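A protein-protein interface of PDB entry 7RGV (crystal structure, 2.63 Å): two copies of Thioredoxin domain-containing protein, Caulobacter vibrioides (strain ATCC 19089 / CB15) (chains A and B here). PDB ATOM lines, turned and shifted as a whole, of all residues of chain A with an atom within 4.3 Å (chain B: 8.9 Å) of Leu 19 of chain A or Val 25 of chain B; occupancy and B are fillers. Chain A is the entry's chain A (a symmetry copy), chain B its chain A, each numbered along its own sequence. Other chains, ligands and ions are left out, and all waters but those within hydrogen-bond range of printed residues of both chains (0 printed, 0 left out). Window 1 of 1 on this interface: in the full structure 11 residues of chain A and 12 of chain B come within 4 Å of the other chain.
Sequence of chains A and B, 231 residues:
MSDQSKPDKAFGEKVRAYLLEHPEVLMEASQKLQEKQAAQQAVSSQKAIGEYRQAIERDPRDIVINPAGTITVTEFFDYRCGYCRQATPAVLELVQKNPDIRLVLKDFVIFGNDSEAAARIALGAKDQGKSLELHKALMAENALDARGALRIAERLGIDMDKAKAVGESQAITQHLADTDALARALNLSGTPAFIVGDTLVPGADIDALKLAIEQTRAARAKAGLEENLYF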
ATOM      1  N   VAL A  15     -20.343  31.603 -27.840  1.00  0.00           N
ATOM      2  CA  VAL A  15     -19.524  30.980 -28.878  1.00  0.00           C
ATOM      3  C   VAL A  15     -19.697  29.467 -28.845  1.00  0.00           C
ATOM      4  O   VAL A  15     -19.924  28.826 -29.877  1.00  0.00           O
ATOM      5  CB  VAL A  15     -18.046  31.373 -28.710  1.00  0.00           C
ATOM      6  CG1 VAL A  15     -17.172  30.541 -29.643  1.00  0.00           C
ATOM      7  CG2 VAL A  15     -17.852  32.850 -28.980  1.00  0.00           C
ATOM      8  N   ARG A  16     -19.583  28.875 -27.655  1.00  0.00           N
ATOM      9  CA  ARG A  16     -19.708  27.427 -27.532  1.00  0.00           C
ATOM     10  C   ARG A  16     -21.091  26.957 -27.967  1.00  0.00           C
ATOM     11  O   ARG A  16     -21.218  25.958 -28.685  1.00  0.00           O
ATOM     12  CB  ARG A  16     -19.422  27.005 -26.090  1.00  0.00           C
ATOM     13  CG  ARG A  16     -19.396  25.505 -25.868  1.00  0.00           C
ATOM     14  CD  ARG A  16     -18.995  25.161 -24.439  1.00  0.00           C
ATOM     15  NE  ARG A  16     -19.368  23.795 -24.089  1.00  0.00           N
ATOM     16  CZ  ARG A  16     -20.523  23.454 -23.531  1.00  0.00           C
ATOM     17  NH1 ARG A  16     -21.439  24.358 -23.229  1.00  0.00           N
ATOM     18  NH2 ARG A  16     -20.763  22.172 -23.270  1.00  0.00           N
ATOM     19  N   ALA A  17     -22.137  27.672 -27.548  1.00  0.00           N
ATOM     20  CA  ALA A  17     -23.495  27.301 -27.928  1.00  0.00           C
ATOM     21  C   ALA A  17     -23.648  27.258 -29.442  1.00  0.00           C
ATOM     22  O   ALA A  17     -24.187  26.294 -29.999  1.00  0.00           O
ATOM     23  CB  ALA A  17     -24.495  28.287 -27.324  1.00  0.00           C
ATOM     24  N   TYR A  18     -23.193  28.308 -30.128  1.00  0.00           N
ATOM     25  CA  TYR A  18     -23.287  28.330 -31.582  1.00  0.00           C
ATOM     26  C   TYR A  18     -22.554  27.143 -32.192  1.00  0.00           C
ATOM     27  O   TYR A  18     -23.113  26.405 -33.012  1.00  0.00           O
ATOM     28  CB  TYR A  18     -22.723  29.640 -32.127  1.00  0.00           C
ATOM     29  CG  TYR A  18     -22.752  29.709 -33.635  1.00  0.00           C
ATOM     30  CD1 TYR A  18     -23.938  29.955 -34.310  1.00  0.00           C
ATOM     31  CD2 TYR A  18     -21.598  29.518 -34.383  1.00  0.00           C
ATOM     32  CE1 TYR A  18     -23.978  30.014 -35.686  1.00  0.00           C
ATOM     33  CE2 TYR A  18     -21.627  29.577 -35.765  1.00  0.00           C
ATOM     34  CZ  TYR A  18     -22.822  29.825 -36.409  1.00  0.00           C
ATOM     35  OH  TYR A  18     -22.866  29.885 -37.781  1.00  0.00           O
ATOM     36  N   LEU A  19     -21.295  26.939 -31.798  1.00  0.00           N
ATOM     37  CA  LEU A  19     -20.499  25.879 -32.408  1.00  0.00           C
ATOM     38  C   LEU A  19     -21.143  24.516 -32.201  1.00  0.00           C
ATOM     39  O   LEU A  19     -21.141  23.677 -33.109  1.00  0.00           O
ATOM     40  CB  LEU A  19     -19.085  25.890 -31.834  1.00  0.00           C
ATOM     41  CG  LEU A  19     -18.264  27.127 -32.189  1.00  0.00           C
ATOM     42  CD1 LEU A  19     -16.929  27.096 -31.472  1.00  0.00           C
ATOM     43  CD2 LEU A  19     -18.068  27.218 -33.693  1.00  0.00           C
ATOM     44  N   LEU A  20     -21.697  24.273 -31.012  1.00  0.00           N
ATOM     45  CA  LEU A  20     -22.319  22.982 -30.751  1.00  0.00           C
ATOM     46  C   LEU A  20     -23.622  22.827 -31.522  1.00  0.00           C
ATOM     47  O   LEU A  20     -23.972  21.712 -31.931  1.00  0.00           O
ATOM     48  CB  LEU A  20     -22.572  22.810 -29.255  1.00  0.00           C
ATOM     49  CG  LEU A  20     -21.318  22.730 -28.382  1.00  0.00           C
ATOM     50  CD1 LEU A  20     -21.703  22.613 -26.914  1.00  0.00           C
ATOM     51  CD2 LEU A  20     -20.435  21.561 -28.804  1.00  0.00           C
ATOM     52  N   GLU A  21     -24.345  23.925 -31.733  1.00  0.00           N
ATOM     53  CA  GLU A  21     -25.602  23.889 -32.465  1.00  0.00           C
ATOM     54  C   GLU A  21     -25.411  23.979 -33.971  1.00  0.00           C
ATOM     55  O   GLU A  21     -26.316  23.595 -34.720  1.00  0.00           O
ATOM     56  CB  GLU A  21     -26.510  25.025 -31.994  1.00  0.00           C
ATOM     57  CG  GLU A  21     -27.060  24.798 -30.600  1.00  0.00           C
ATOM     58  CD  GLU A  21     -27.808  23.488 -30.507  1.00  0.00           C
ATOM     59  OE1 GLU A  21     -28.463  23.122 -31.506  1.00  0.00           O
ATOM     60  OE2 GLU A  21     -27.724  22.810 -29.461  1.00  0.00           O
ATOM     61  N   HIS A  22     -24.261  24.467 -34.431  1.00  0.00           N
ATOM     62  CA  HIS A  22     -23.939  24.503 -35.859  1.00  0.00           C
ATOM     63  C   HIS A  22     -22.489  24.075 -36.043  1.00  0.00           C
ATOM     64  O   HIS A  22     -21.643  24.847 -36.502  1.00  0.00           O
ATOM     65  CB  HIS A  22     -24.203  25.892 -36.432  1.00  0.00           C
ATOM     66  CG  HIS A  22     -25.593  26.386 -36.174  1.00  0.00           C
ATOM     67  ND1 HIS A  22     -26.696  25.874 -36.825  1.00  0.00           N
ATOM     68  CD2 HIS A  22     -26.062  27.327 -35.322  1.00  0.00           C
ATOM     69  CE1 HIS A  22     -27.783  26.486 -36.391  1.00  0.00           C
ATOM     70  NE2 HIS A  22     -27.425  27.372 -35.478  1.00  0.00           N
ATOM     71  N   PRO A  23     -22.170  22.826 -35.686  1.00  0.00           N
ATOM     72  CA  PRO A  23     -20.788  22.346 -35.832  1.00  0.00           C
ATOM     73  C   PRO A  23     -20.337  22.223 -37.273  1.00  0.00           C
ATOM     74  O   PRO A  23     -19.143  21.994 -37.510  1.00  0.00           O
ATOM     75  CB  PRO A  23     -20.816  20.975 -35.144  1.00  0.00           C
ATOM     76  CG  PRO A  23     -22.234  20.520 -35.291  1.00  0.00           C
ATOM     77  CD  PRO A  23     -23.078  21.769 -35.198  1.00  0.00           C
ATOM     78  N   VAL B  15     -13.216  35.615 -29.920  1.00  0.00           N
ATOM     79  CA  VAL B  15     -13.529  34.258 -30.364  1.00  0.00           C
ATOM     80  C   VAL B  15     -12.280  33.389 -30.315  1.00  0.00           C
ATOM     81  O   VAL B  15     -12.296  32.272 -29.784  1.00  0.00           O
ATOM     82  CB  VAL B  15     -14.138  34.276 -31.777  1.00  0.00           C
ATOM     83  CG1 VAL B  15     -14.243  32.857 -32.322  1.00  0.00           C
ATOM     84  CG2 VAL B  15     -15.499  34.941 -31.764  1.00  0.00           C
ATOM     85  N   TYR B  18     -11.157  32.540 -26.677  1.00  0.00           N
ATOM     86  CA  TYR B  18     -11.966  31.485 -26.079  1.00  0.00           C
ATOM     87  C   TYR B  18     -11.574  30.121 -26.630  1.00  0.00           C
ATOM     88  O   TYR B  18     -11.307  29.183 -25.868  1.00  0.00           O
ATOM     89  CB  TYR B  18     -13.449  31.753 -26.326  1.00  0.00           C
ATOM     90  CG  TYR B  18     -14.341  30.673 -25.765  1.00  0.00           C
ATOM     91  CD1 TYR B  18     -14.596  30.599 -24.404  1.00  0.00           C
ATOM     92  CD2 TYR B  18     -14.919  29.720 -26.593  1.00  0.00           C
ATOM     93  CE1 TYR B  18     -15.404  29.613 -23.880  1.00  0.00           C
ATOM     94  CE2 TYR B  18     -15.733  28.728 -26.077  1.00  0.00           C
ATOM     95  CZ  TYR B  18     -15.970  28.681 -24.719  1.00  0.00           C
ATOM     96  OH  TYR B  18     -16.776  27.700 -24.192  1.00  0.00           O
ATOM     97  N   LEU B  19     -11.530  29.991 -27.957  1.00  0.00           N
ATOM     98  CA  LEU B  19     -11.254  28.691 -28.558  1.00  0.00           C
ATOM     99  C   LEU B  19      -9.898  28.156 -28.120  1.00  0.00           C
ATOM    100  O   LEU B  19      -9.751  26.957 -27.860  1.00  0.00           O
ATOM    101  CB  LEU B  19     -11.318  28.793 -30.079  1.00  0.00           C
ATOM    102  CG  LEU B  19     -12.706  29.096 -30.638  1.00  0.00           C
ATOM    103  CD1 LEU B  19     -12.637  29.298 -32.138  1.00  0.00           C
ATOM    104  CD2 LEU B  19     -13.674  27.979 -30.287  1.00  0.00           C
ATOM    105  N   LEU B  20      -8.893  29.029 -28.037  1.00  0.00           N
ATOM    106  CA  LEU B  20      -7.568  28.574 -27.632  1.00  0.00           C
ATOM    107  C   LEU B  20      -7.533  28.209 -26.157  1.00  0.00           C
ATOM    108  O   LEU B  20      -6.795  27.297 -25.761  1.00  0.00           O
ATOM    109  CB  LEU B  20      -6.527  29.649 -27.934  1.00  0.00           C
ATOM    110  CG  LEU B  20      -6.309  29.956 -29.416  1.00  0.00           C
ATOM    111  CD1 LEU B  20      -5.291  31.077 -29.581  1.00  0.00           C
ATOM    112  CD2 LEU B  20      -5.867  28.708 -30.172  1.00  0.00           C
ATOM    113  N   GLU B  21      -8.317  28.901 -25.333  1.00  0.00           N
ATOM    114  CA  GLU B  21      -8.364  28.628 -23.905  1.00  0.00           C
ATOM    115  C   GLU B  21      -9.330  27.510 -23.550  1.00  0.00           C
ATOM    116  O   GLU B  21      -9.209  26.925 -22.467  1.00  0.00           O
ATOM    117  CB  GLU B  21      -8.747  29.898 -23.145  1.00  0.00           C
ATOM    118  CG  GLU B  21      -7.640  30.933 -23.137  1.00  0.00           C
ATOM    119  CD  GLU B  21      -6.362  30.371 -22.558  1.00  0.00           C
ATOM    120  OE1 GLU B  21      -6.460  29.551 -21.621  1.00  0.00           O
ATOM    121  OE2 GLU B  21      -5.266  30.716 -23.049  1.00  0.00           O
ATOM    122  N   HIS B  22     -10.278  27.193 -24.430  1.00  0.00           N
ATOM    123  CA  HIS B  22     -11.194  26.069 -24.227  1.00  0.00           C
ATOM    124  C   HIS B  22     -11.349  25.323 -25.544  1.00  0.00           C
ATOM    125  O   HIS B  22     -12.438  25.255 -26.121  1.00  0.00           O
ATOM    126  CB  HIS B  22     -12.534  26.560 -23.685  1.00  0.00           C
ATOM    127  CG  HIS B  22     -12.405  27.388 -22.444  1.00  0.00           C
ATOM    128  ND1 HIS B  22     -12.074  26.846 -21.220  1.00  0.00           N
ATOM    129  CD2 HIS B  22     -12.538  28.720 -22.242  1.00  0.00           C
ATOM    130  CE1 HIS B  22     -12.019  27.807 -20.316  1.00  0.00           C
ATOM    131  NE2 HIS B  22     -12.297  28.954 -20.910  1.00  0.00           N
ATOM    132  N   PRO B  23     -10.256  24.743 -26.052  1.00  0.00           N
ATOM    133  CA  PRO B  23     -10.332  24.009 -27.324  1.00  0.00           C
ATOM    134  C   PRO B  23     -11.166  22.746 -27.248  1.00  0.00           C
ATOM    135  O   PRO B  23     -11.437  22.144 -28.295  1.00  0.00           O
ATOM    136  CB  PRO B  23      -8.864  23.685 -27.631  1.00  0.00           C
ATOM    137  CG  PRO B  23      -8.211  23.629 -26.287  1.00  0.00           C
ATOM    138  CD  PRO B  23      -8.913  24.670 -25.446  1.00  0.00           C
ATOM    139  N   GLU B  24     -11.571  22.319 -26.052  1.00  0.00           N
ATOM    140  CA  GLU B  24     -12.429  21.147 -25.940  1.00  0.00           C
ATOM    141  C   GLU B  24     -13.769  21.360 -26.631  1.00  0.00           C
ATOM    142  O   GLU B  24     -14.454  20.380 -26.948  1.00  0.00           O
ATOM    143  CB  GLU B  24     -12.640  20.795 -24.467  1.00  0.00           C
ATOM    144  CG  GLU B  24     -11.375  20.340 -23.739  1.00  0.00           C
ATOM    145  CD  GLU B  24     -10.474  21.491 -23.308  1.00  0.00           C
ATOM    146  OE1 GLU B  24     -10.768  22.654 -23.657  1.00  0.00           O
ATOM    147  OE2 GLU B  24      -9.468  21.226 -22.615  1.00  0.00           O
ATOM    148  N   VAL B  25     -14.153  22.617 -26.875  1.00  0.00           N
ATOM    149  CA  VAL B  25     -15.383  22.891 -27.610  1.00  0.00           C
ATOM    150  C   VAL B  25     -15.333  22.253 -28.991  1.00  0.00           C
ATOM    151  O   VAL B  25     -16.367  21.843 -29.534  1.00  0.00           O
ATOM    152  CB  VAL B  25     -15.619  24.411 -27.713  1.00  0.00           C
ATOM    153  CG1 VAL B  25     -16.888  24.692 -28.503  1.00  0.00           C
ATOM    154  CG2 VAL B  25     -15.683  25.038 -26.329  1.00  0.00           C
ATOM    155  N   LEU B  26     -14.142  22.167 -29.584  1.00  0.00           N
ATOM    156  CA  LEU B  26     -14.013  21.565 -30.907  1.00  0.00           C
ATOM    157  C   LEU B  26     -14.225  20.057 -30.851  1.00  0.00           C
ATOM    158  O   LEU B  26     -14.854  19.481 -31.747  1.00  0.00           O
ATOM    159  CB  LEU B  26     -12.643  21.897 -31.495  1.00  0.00           C
ATOM    160  CG  LEU B  26     -12.311  23.390 -31.545  1.00  0.00           C
ATOM    161  CD1 LEU B  26     -10.926  23.617 -32.131  1.00  0.00           C
ATOM    162  CD2 LEU B  26     -13.357  24.154 -32.338  1.00  0.00           C
ATOM    163  N   MET B  27     -13.705  19.397 -29.814  1.00  0.00           N
ATOM    164  CA  MET B  27     -14.007  17.983 -29.624  1.00  0.00           C
ATOM    165  C   MET B  27     -15.509  17.769 -29.467  1.00  0.00           C
ATOM    166  O   MET B  27     -16.083  16.854 -30.069  1.00  0.00           O
ATOM    167  CB  MET B  27     -13.261  17.443 -28.405  1.00  0.00           C
ATOM    168  CG  MET B  27     -11.744  17.534 -28.495  1.00  0.00           C
ATOM    169  SD  MET B  27     -11.033  16.505 -29.798  1.00  0.00           S
ATOM    170  CE  MET B  27     -10.813  17.702 -31.116  1.00  0.00           C
ATOM    171  N   GLU B  28     -16.164  18.615 -28.667  1.00  0.00           N
ATOM    172  CA  GLU B  28     -17.602  18.474 -28.460  1.00  0.00           C
ATOM    173  C   GLU B  28     -18.368  18.652 -29.764  1.00  0.00           C
ATOM    174  O   GLU B  28     -19.308  17.900 -30.048  1.00  0.00           O
ATOM    175  CB  GLU B  28     -18.078  19.485 -27.417  1.00  0.00           C
ATOM    176  CG  GLU B  28     -17.512  19.259 -26.026  1.00  0.00           C
ATOM    177  CD  GLU B  28     -17.704  20.458 -25.117  1.00  0.00           C
ATOM    178  OE1 GLU B  28     -18.629  21.261 -25.369  1.00  0.00           O
ATOM    179  OE2 GLU B  28     -16.922  20.605 -24.152  1.00  0.00           O
ATOM    180  N   ALA B  29     -17.986  19.648 -30.569  1.00  0.00           N
ATOM    181  CA  ALA B  29     -18.640  19.847 -31.858  1.00  0.00           C
ATOM    182  C   ALA B  29     -18.352  18.691 -32.808  1.00  0.00           C
ATOM    183  O   ALA B  29     -19.233  18.265 -33.564  1.00  0.00           O
ATOM    184  CB  ALA B  29     -18.189  21.170 -32.475  1.00  0.00           C
ATOM    185  N   SER B  30     -17.122  18.174 -32.789  1.00  0.00           N
ATOM    186  CA  SER B  30     -16.798  17.022 -33.622  1.00  0.00           C
ATOM    187  C   SER B  30     -17.635  15.813 -33.224  1.00  0.00           C
ATOM    188  O   SER B  30     -18.053  15.028 -34.082  1.00  0.00           O
ATOM    189  CB  SER B  30     -15.307  16.704 -33.520  1.00  0.00           C
ATOM    190  OG  SER B  30     -14.974  15.569 -34.301  1.00  0.00           O
ATOM    191  N   GLN B  31     -17.893  15.649 -31.923  1.00  0.00           N
ATOM    192  CA  GLN B  31     -18.744  14.552 -31.474  1.00  0.00           C
ATOM    193  C   GLN B  31     -20.169  14.722 -31.987  1.00  0.00           C
ATOM    194  O   GLN B  31     -20.801  13.749 -32.416  1.00  0.00           O
ATOM    195  CB  GLN B  31     -18.719  14.465 -29.947  1.00  0.00           C
ATOM    196  CG  GLN B  31     -19.639  13.404 -29.353  1.00  0.00           C
ATOM    197  CD  GLN B  31     -19.203  11.985 -29.679  1.00  0.00           C
ATOM    198  OE1 GLN B  31     -18.014  11.706 -29.842  1.00  0.00           O
ATOM    199  NE2 GLN B  31     -20.170  11.078 -29.776  1.00  0.00           N
ATOM    200  N   LYS B  32     -20.696  15.950 -31.945  1.00  0.00           N
ATOM    201  CA  LYS B  32     -22.021  16.206 -32.503  1.00  0.00           C
ATOM    202  C   LYS B  32     -22.076  15.794 -33.971  1.00  0.00           C
ATOM    203  O   LYS B  32     -23.025  15.135 -34.411  1.00  0.00           O
ATOM    204  CB  LYS B  32     -22.383  17.686 -32.348  1.00  0.00           C
ATOM    205  CG  LYS B  32     -22.507  18.176 -30.908  1.00  0.00           C
ATOM    206  CD  LYS B  32     -23.815  17.739 -30.263  1.00  0.00           C
ATOM    207  CE  LYS B  32     -24.011  18.413 -28.911  1.00  0.00           C
ATOM    208  NZ  LYS B  32     -25.143  17.823 -28.141  1.00  0.00           N
ATOM    209  N   LEU B  33     -21.054  16.170 -34.745  1.00  0.00           N
ATOM    210  CA  LEU B  33     -21.038  15.834 -36.164  1.00  0.00           C
ATOM    211  C   LEU B  33     -20.970  14.328 -36.376  1.00  0.00           C
ATOM    212  O   LEU B  33     -21.595  13.793 -37.300  1.00  0.00           O
ATOM    213  CB  LEU B  33     -19.858  16.520 -36.850  1.00  0.00           C
ATOM    214  CG  LEU B  33     -20.130  17.901 -37.444  1.00  0.00           C
ATOM    215  CD1 LEU B  33     -18.825  18.605 -37.763  1.00  0.00           C
ATOM    216  CD2 LEU B  33     -20.988  17.785 -38.693  1.00  0.00           C
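Leu 19 of chain A touches just these residues of chain B: Leu 19 (3.6 Å), Val 25 (3.8 Å) and Ala 29 (3.9 Å).
Printed residues of chain B within 4 Å of Pro 23 of chain A: Ala 29 and Leu 33.
Printed residues of chain A within 4 Å of Leu 19 of chain B: Leu 19.
Val 25 of chain B touches just these residues of chain A: Arg 16 (3.7 Å) and Leu 19 (3.8 Å).
Printed residues of chain A within 4 Å of Glu 28 of chain B: Arg 16 (2.9 Å) and Leu 20 (3.4 Å).
The nearest residue of chain A that does not touch Val 25 of chain B is Leu 20 of chain A (4.1 Å).
The side-chain carboxylate (OE1) of Glu 28 of chain B is in salt-bridge range of the guanidinium group (NE) of Arg 16 of chain A, 2.9 Å away.
Of the 17 printed residues of chain B, 7 touch a printed residue of chain A.
Of the 9 printed residues of chain A, 5 touch a printed residue of chain B.
Hydrophobic or aromatic side chains of chain A within 4 Å of the printed part of chain B: Val 15, Leu 19, Leu 20 and Pro 23.
Among the printed residues, Asp or Glu carboxylates within 4 Å of a Lys or Arg side-chain nitrogen of the other chain: Arg 16 of chain A with Glu 28 of chain B (2.9 Å).
Val 15 of chain A touches Tyr 18 of chain B, but with the chains exchanged Tyr 18 of chain A does not touch Val 15 of chain B (8.3 Å).
Leu 19 of chain A touches its own counterpart, Leu 19 of chain B.
Of the 12 pairs that touch across the chains among the printed residues, 1 has its exchanged pair printed and touching as well.
CD2 of Tyr 18 of chain B touches CG1 of Val 15 of chain A (3.9 Å).
CB of Arg 16 of chain A touches OH of Tyr 18 of chain B, 3.3 Å away.
Arg 16 of chain A touches Val 25 of chain B.
CD2 of Leu 19 of chain B touches CD1 of Leu 19 of chain A (3.6 Å).
Leu 19 of chain A touches Val 25 of chain B (CD1 to CG1, 3.8 Å).
O of Leu 19 of chain A touches CB of Ala 29 of chain B, 3.9 Å away.
Leu 20 of chain A touches Glu 28 of chain B.
N of Ala 29 of chain B touches CD2 of Leu 20 of chain A, at 3.6 Å.
Lys 32 of chain B touches Leu 20 of chain A (CG to O, 3.96 Å).
Pro 23 of chain A touches Ala 29 of chain B.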
